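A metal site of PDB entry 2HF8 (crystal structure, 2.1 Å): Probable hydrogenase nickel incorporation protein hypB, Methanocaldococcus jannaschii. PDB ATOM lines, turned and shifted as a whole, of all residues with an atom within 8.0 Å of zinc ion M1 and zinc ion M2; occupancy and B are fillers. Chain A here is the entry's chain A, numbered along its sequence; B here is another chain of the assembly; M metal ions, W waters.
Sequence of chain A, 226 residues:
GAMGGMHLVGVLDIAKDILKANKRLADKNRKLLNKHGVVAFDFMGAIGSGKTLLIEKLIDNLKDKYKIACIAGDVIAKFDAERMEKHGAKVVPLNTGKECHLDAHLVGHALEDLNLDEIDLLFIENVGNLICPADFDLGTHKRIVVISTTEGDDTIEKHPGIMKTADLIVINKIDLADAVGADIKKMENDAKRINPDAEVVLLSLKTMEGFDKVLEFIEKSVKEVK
SG of Cys 100 of chain B is bound to zinc ion M2 (2.1 Å).
ND1 of His 101 of chain B binds zinc ion M2 (2.2 Å).
Zinc ion M2 is bound by water W1, at 2.2 Å.
The side-chain sulfur (SG) of Cys 132 of chain B binds zinc ion M2 (2.3 Å).
O of Cys 100 of chain B lies within hydrogen-bond range of ND2 of Asn 129 of chain B (3.1 Å).
NE2 of His 101 of chain B lies close to OE2 of Glu 99 of chain B.
The backbone NH of Cys 132 of chain A sits at hydrogen-bond distance from the side-chain amide oxygen of Asn 129 of chain A (3.4 Å).
The side-chain sulfur (SG) of Cys 132 of chain B sits close to the side-chain amide nitrogen (ND2) of Asn 129 of chain B, 3.6 Å away.
O of Cys 100 of chain A lies within hydrogen-bond range of ND2 of Asn 129 of chain A, at 2.8 Å.
Zinc ion M1 is bound by the side-chain sulfur (SG) of Cys 132 of chain A (2.2 Å), the side-chain sulfur (SG) of Cys 100 of chain B (2.2 Å) and the side-chain sulfur (SG) of Cys 100 of chain A (2.4 Å).
The nearest printed residue that does not touch zinc ion M2 is Cys 100 of chain A (4.3 Å).
Three residues have an atom within 4 Å of zinc ion M1: Cys 100 of chain A, Cys 132 of chain A and Cys 100 of chain B.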
ATOM      1  N   LYS A  98     -12.483  -6.545  21.831  1.00  0.00           N
ATOM      2  CA  LYS A  98     -11.709  -6.071  20.691  1.00  0.00           C
ATOM      3  C   LYS A  98     -10.753  -4.930  21.040  1.00  0.00           C
ATOM      4  O   LYS A  98      -9.944  -4.509  20.212  1.00  0.00           O
ATOM      5  CB  LYS A  98     -12.632  -5.680  19.523  1.00  0.00           C
ATOM      6  CG  LYS A  98     -13.219  -6.869  18.774  1.00  0.00           C
ATOM      7  CD  LYS A  98     -13.877  -6.432  17.469  1.00  0.00           C
ATOM      8  CE  LYS A  98     -14.233  -7.631  16.612  1.00  0.00           C
ATOM      9  NZ  LYS A  98     -14.872  -7.226  15.323  1.00  0.00           N
ATOM     10  N   GLU A  99     -10.845  -4.436  22.280  1.00  0.00           N
ATOM     11  CA  GLU A  99      -9.993  -3.348  22.765  1.00  0.00           C
ATOM     12  C   GLU A  99      -8.561  -3.838  23.003  1.00  0.00           C
ATOM     13  O   GLU A  99      -8.339  -4.941  23.498  1.00  0.00           O
ATOM     14  CB  GLU A  99     -10.565  -2.758  24.047  1.00  0.00           C
ATOM     15  CG  GLU A  99     -10.057  -1.352  24.385  1.00  0.00           C
ATOM     16  CD  GLU A  99     -11.015  -0.247  23.948  1.00  0.00           C
ATOM     17  OE1 GLU A  99     -11.715  -0.397  22.913  1.00  0.00           O
ATOM     18  OE2 GLU A  99     -11.062   0.785  24.660  1.00  0.00           O
ATOM     19  N   CYS A 100      -7.582  -3.006  22.645  1.00  0.00           N
ATOM     20  CA  CYS A 100      -6.172  -3.384  22.711  1.00  0.00           C
ATOM     21  C   CYS A 100      -5.477  -2.888  23.983  1.00  0.00           C
ATOM     22  O   CYS A 100      -4.254  -2.995  24.114  1.00  0.00           O
ATOM     23  CB  CYS A 100      -5.436  -2.906  21.455  1.00  0.00           C
ATOM     24  SG  CYS A 100      -5.837  -1.213  20.938  1.00  0.00           S
ATOM     25  N   HIS A 101      -6.257  -2.368  24.920  1.00  0.00           N
ATOM     26  CA  HIS A 101      -5.744  -1.810  26.174  1.00  0.00           C
ATOM     27  C   HIS A 101      -6.842  -1.699  27.232  1.00  0.00           C
ATOM     28  O   HIS A 101      -8.026  -1.689  26.905  1.00  0.00           O
ATOM     29  CB  HIS A 101      -5.141  -0.412  25.923  1.00  0.00           C
ATOM     30  CG  HIS A 101      -6.154   0.597  25.488  1.00  0.00           C
ATOM     31  ND1 HIS A 101      -6.502   0.781  24.158  1.00  0.00           N
ATOM     32  CD2 HIS A 101      -6.920   1.456  26.204  1.00  0.00           C
ATOM     33  CE1 HIS A 101      -7.426   1.717  24.082  1.00  0.00           C
ATOM     34  NE2 HIS A 101      -7.704   2.142  25.305  1.00  0.00           N
ATOM     35  N   ASN A 129       0.295  -6.798  25.423  1.00  0.00           N
ATOM     36  CA  ASN A 129       0.454  -5.753  24.400  1.00  0.00           C
ATOM     37  C   ASN A 129       1.591  -4.830  24.836  1.00  0.00           C
ATOM     38  O   ASN A 129       1.544  -4.262  25.926  1.00  0.00           O
ATOM     39  CB  ASN A 129      -0.857  -4.963  24.247  1.00  0.00           C
ATOM     40  CG  ASN A 129      -0.872  -4.044  23.023  1.00  0.00           C
ATOM     41  OD1 ASN A 129       0.170  -3.602  22.543  1.00  0.00           O
ATOM     42  ND2 ASN A 129      -2.067  -3.753  22.537  1.00  0.00           N
ATOM     43  N   ILE A 131       2.505  -2.089  23.209  1.00  0.00           N
ATOM     44  CA  ILE A 131       2.330  -0.810  22.534  1.00  0.00           C
ATOM     45  C   ILE A 131       1.325   0.082  23.267  1.00  0.00           C
ATOM     46  O   ILE A 131       1.726   1.023  23.956  1.00  0.00           O
ATOM     47  CB  ILE A 131       1.937  -1.002  21.037  1.00  0.00           C
ATOM     48  CG1 ILE A 131       3.040  -1.792  20.312  1.00  0.00           C
ATOM     49  CG2 ILE A 131       1.700   0.356  20.364  1.00  0.00           C
ATOM     50  CD1 ILE A 131       2.697  -2.270  18.921  1.00  0.00           C
ATOM     51  N   CYS A 132       0.042  -0.222  23.134  1.00  0.00           N
ATOM     52  CA  CYS A 132      -1.053   0.656  23.565  1.00  0.00           C
ATOM     53  C   CYS A 132      -1.083   0.997  25.068  1.00  0.00           C
ATOM     54  O   CYS A 132      -1.341   2.147  25.428  1.00  0.00           O
ATOM     55  CB  CYS A 132      -2.410   0.104  23.107  1.00  0.00           C
ATOM     56  SG  CYS A 132      -2.336  -0.760  21.518  1.00  0.00           S
ATOM     57  N   PRO A 133      -0.851   0.000  25.959  1.00  0.00           N
ATOM     58  CA  PRO A 133      -0.870   0.312  27.398  1.00  0.00           C
ATOM     59  C   PRO A 133       0.089   1.417  27.890  1.00  0.00           C
ATOM     60  O   PRO A 133      -0.081   1.920  28.997  1.00  0.00           O
ATOM     61  CB  PRO A 133      -0.516  -1.039  28.050  1.00  0.00           C
ATOM     62  CG  PRO A 133      -0.960  -2.050  27.046  1.00  0.00           C
ATOM     63  CD  PRO A 133      -0.622  -1.435  25.724  1.00  0.00           C
ATOM     64  N   ASP A 135       0.233   4.469  26.925  1.00  0.00           N
ATOM     65  CA  ASP A 135      -0.475   5.765  26.987  1.00  0.00           C
ATOM     66  C   ASP A 135      -1.616   5.812  28.020  1.00  0.00           C
ATOM     67  O   ASP A 135      -2.151   6.889  28.292  1.00  0.00           O
ATOM     68  CB  ASP A 135      -1.044   6.132  25.620  1.00  0.00           C
ATOM     69  CG  ASP A 135       0.020   6.144  24.519  1.00  0.00           C
ATOM     70  OD1 ASP A 135       1.117   6.705  24.737  1.00  0.00           O
ATOM     71  OD2 ASP A 135      -0.275   5.600  23.425  1.00  0.00           O
ATOM     72  N   PHE A 136      -1.980   4.667  28.590  1.00  0.00           N
ATOM     73  CA  PHE A 136      -3.173   4.577  29.432  1.00  0.00           C
ATOM     74  C   PHE A 136      -2.917   4.251  30.911  1.00  0.00           C
ATOM     75  O   PHE A 136      -3.041   3.110  31.342  1.00  0.00           O
ATOM     76  CB  PHE A 136      -4.187   3.602  28.814  1.00  0.00           C
ATOM     77  CG  PHE A 136      -4.799   4.099  27.546  1.00  0.00           C
ATOM     78  CD1 PHE A 136      -4.243   3.770  26.308  1.00  0.00           C
ATOM     79  CD2 PHE A 136      -5.945   4.907  27.572  1.00  0.00           C
ATOM     80  CE1 PHE A 136      -4.815   4.245  25.121  1.00  0.00           C
ATOM     81  CE2 PHE A 136      -6.517   5.382  26.386  1.00  0.00           C
ATOM     82  CZ  PHE A 136      -5.957   5.049  25.161  1.00  0.00           C
ATOM     83  N   LYS B  98       2.855   4.718  17.123  1.00  0.00           N
ATOM     84  CA  LYS B  98       2.078   4.307  18.286  1.00  0.00           C
ATOM     85  C   LYS B  98       0.847   3.512  17.858  1.00  0.00           C
ATOM     86  O   LYS B  98       0.070   3.052  18.696  1.00  0.00           O
ATOM     87  CB  LYS B  98       1.699   5.509  19.155  1.00  0.00           C
ATOM     88  CG  LYS B  98       2.789   5.923  20.126  1.00  0.00           C
ATOM     89  CD  LYS B  98       2.310   6.995  21.081  1.00  0.00           C
ATOM     90  CE  LYS B  98       3.322   7.260  22.194  1.00  0.00           C
ATOM     91  NZ  LYS B  98       4.625   7.789  21.703  1.00  0.00           N
ATOM     92  N   GLU B  99       0.686   3.364  16.540  1.00  0.00           N
ATOM     93  CA  GLU B  99      -0.366   2.533  15.968  1.00  0.00           C
ATOM     94  C   GLU B  99      -0.016   1.069  16.183  1.00  0.00           C
ATOM     95  O   GLU B  99       1.146   0.678  16.120  1.00  0.00           O
ATOM     96  CB  GLU B  99      -0.563   2.853  14.484  1.00  0.00           C
ATOM     97  CG  GLU B  99      -1.917   2.433  13.911  1.00  0.00           C
ATOM     98  CD  GLU B  99      -3.080   3.268  14.408  1.00  0.00           C
ATOM     99  OE1 GLU B  99      -2.882   4.460  14.765  1.00  0.00           O
ATOM    100  OE2 GLU B  99      -4.220   2.742  14.441  1.00  0.00           O
ATOM    101  N   CYS B 100      -1.043   0.261  16.425  1.00  0.00           N
ATOM    102  CA  CYS B 100      -0.873  -1.106  16.919  1.00  0.00           C
ATOM    103  C   CYS B 100      -1.208  -2.153  15.871  1.00  0.00           C
ATOM    104  O   CYS B 100      -1.286  -3.344  16.184  1.00  0.00           O
ATOM    105  CB  CYS B 100      -1.740  -1.300  18.157  1.00  0.00           C
ATOM    106  SG  CYS B 100      -3.263  -0.306  18.115  1.00  0.00           S
ATOM    107  N   HIS B 101      -1.393  -1.708  14.626  1.00  0.00           N
ATOM    108  CA  HIS B 101      -1.755  -2.582  13.520  1.00  0.00           C
ATOM    109  C   HIS B 101      -1.426  -1.932  12.180  1.00  0.00           C
ATOM    110  O   HIS B 101      -1.429  -0.700  12.056  1.00  0.00           O
ATOM    111  CB  HIS B 101      -3.256  -2.916  13.574  1.00  0.00           C
ATOM    112  CG  HIS B 101      -4.146  -1.716  13.519  1.00  0.00           C
ATOM    113  ND1 HIS B 101      -4.722  -1.165  14.640  1.00  0.00           N
ATOM    114  CD2 HIS B 101      -4.558  -0.952  12.471  1.00  0.00           C
ATOM    115  CE1 HIS B 101      -5.443  -0.111  14.297  1.00  0.00           C
ATOM    116  NE2 HIS B 101      -5.351   0.037  12.982  1.00  0.00           N
ATOM    117  N   LEU B 102      -1.134  -2.756  11.177  1.00  0.00           N
ATOM    118  CA  LEU B 102      -1.102  -2.279   9.801  1.00  0.00           C
ATOM    119  C   LEU B 102      -2.533  -2.121   9.285  1.00  0.00           C
ATOM    120  O   LEU B 102      -3.462  -2.753   9.812  1.00  0.00           O
ATOM    121  CB  LEU B 102      -0.307  -3.234   8.900  1.00  0.00           C
ATOM    122  CG  LEU B 102       1.214  -3.307   9.071  1.00  0.00           C
ATOM    123  CD1 LEU B 102       1.794  -4.331   8.117  1.00  0.00           C
ATOM    124  CD2 LEU B 102       1.875  -1.951   8.843  1.00  0.00           C
ATOM    125  N   VAL B 127       2.296  -6.043  12.610  1.00  0.00           N
ATOM    126  CA  VAL B 127       2.786  -5.722  13.953  1.00  0.00           C
ATOM    127  C   VAL B 127       2.485  -6.878  14.905  1.00  0.00           C
ATOM    128  O   VAL B 127       1.438  -7.526  14.780  1.00  0.00           O
ATOM    129  CB  VAL B 127       2.137  -4.407  14.503  1.00  0.00           C
ATOM    130  CG1 VAL B 127       2.855  -3.924  15.750  1.00  0.00           C
ATOM    131  CG2 VAL B 127       2.142  -3.317  13.450  1.00  0.00           C
ATOM    132  N   ASN B 129       0.957  -8.515  17.623  1.00  0.00           N
ATOM    133  CA  ASN B 129      -0.315  -8.148  18.234  1.00  0.00           C
ATOM    134  C   ASN B 129      -1.369  -9.171  17.854  1.00  0.00           C
ATOM    135  O   ASN B 129      -1.587  -9.443  16.677  1.00  0.00           O
ATOM    136  CB  ASN B 129      -0.746  -6.748  17.756  1.00  0.00           C
ATOM    137  CG  ASN B 129      -1.768  -6.091  18.668  1.00  0.00           C
ATOM    138  OD1 ASN B 129      -2.674  -6.746  19.197  1.00  0.00           O
ATOM    139  ND2 ASN B 129      -1.643  -4.777  18.857  1.00  0.00           N
ATOM    140  N   ILE B 131      -4.629  -8.911  18.831  1.00  0.00           N
ATOM    141  CA  ILE B 131      -5.953  -8.311  18.980  1.00  0.00           C
ATOM    142  C   ILE B 131      -6.428  -7.642  17.686  1.00  0.00           C
ATOM    143  O   ILE B 131      -7.147  -8.249  16.899  1.00  0.00           O
ATOM    144  CB  ILE B 131      -6.015  -7.280  20.155  1.00  0.00           C
ATOM    145  CG1 ILE B 131      -5.357  -7.825  21.427  1.00  0.00           C
ATOM    146  CG2 ILE B 131      -7.462  -6.826  20.410  1.00  0.00           C
ATOM    147  CD1 ILE B 131      -5.844  -9.186  21.879  1.00  0.00           C
ATOM    148  N   CYS B 132      -6.013  -6.395  17.482  1.00  0.00           N
ATOM    149  CA  CYS B 132      -6.599  -5.547  16.450  1.00  0.00           C
ATOM    150  C   CYS B 132      -6.240  -5.848  14.986  1.00  0.00           C
ATOM    151  O   CYS B 132      -7.034  -5.510  14.098  1.00  0.00           O
ATOM    152  CB  CYS B 132      -6.385  -4.058  16.767  1.00  0.00           C
ATOM    153  SG  CYS B 132      -4.755  -3.625  17.389  1.00  0.00           S
ATOM    154  N   PRO B 133      -5.073  -6.482  14.712  1.00  0.00           N
ATOM    155  CA  PRO B 133      -4.841  -6.910  13.320  1.00  0.00           C
ATOM    156  C   PRO B 133      -5.939  -7.797  12.720  1.00  0.00           C
ATOM    157  O   PRO B 133      -6.047  -7.876  11.492  1.00  0.00           O
ATOM    158  CB  PRO B 133      -3.516  -7.683  13.419  1.00  0.00           C
ATOM    159  CG  PRO B 133      -2.818  -7.059  14.568  1.00  0.00           C
ATOM    160  CD  PRO B 133      -3.908  -6.784  15.563  1.00  0.00           C
ATOM    161  N   ASP B 135      -9.013  -7.120  12.698  1.00  0.00           N
ATOM    162  CA  ASP B 135     -10.059  -6.240  12.183  1.00  0.00           C
ATOM    163  C   ASP B 135      -9.680  -5.537  10.884  1.00  0.00           C
ATOM    164  O   ASP B 135     -10.543  -4.928  10.236  1.00  0.00           O
ATOM    165  CB  ASP B 135     -10.432  -5.198  13.248  1.00  0.00           C
ATOM    166  CG  ASP B 135     -11.229  -5.783  14.400  1.00  0.00           C
ATOM    167  OD1 ASP B 135     -11.027  -5.329  15.548  1.00  0.00           O
ATOM    168  OD2 ASP B 135     -12.053  -6.708  14.158  1.00  0.00           O
ATOM    169  N   PHE B 136      -8.402  -5.598  10.519  1.00  0.00           N
ATOM    170  CA  PHE B 136      -7.874  -4.792   9.410  1.00  0.00           C
ATOM    171  C   PHE B 136      -7.280  -5.606   8.258  1.00  0.00           C
ATOM    172  O   PHE B 136      -6.078  -5.879   8.226  1.00  0.00           O
ATOM    173  CB  PHE B 136      -6.874  -3.757   9.941  1.00  0.00           C
ATOM    174  CG  PHE B 136      -7.489  -2.740  10.874  1.00  0.00           C
ATOM    175  CD1 PHE B 136      -7.596  -3.000  12.235  1.00  0.00           C
ATOM    176  CD2 PHE B 136      -7.966  -1.531  10.381  1.00  0.00           C
ATOM    177  CE1 PHE B 136      -8.170  -2.076  13.094  1.00  0.00           C
ATOM    178  CE2 PHE B 136      -8.536  -0.595  11.234  1.00  0.00           C
ATOM    179  CZ  PHE B 136      -8.651  -0.864  12.588  1.00  0.00           C
HETATM  180 ZN    ZN M   1      -3.923  -0.002  20.197  1.00  0.00          ZN
HETATM  181 ZN    ZN M   2      -4.509  -1.380  16.816  1.00  0.00          ZN
HETATM  182  O   HOH W   1      -6.319  -0.427  17.675  1.00  0.00           O
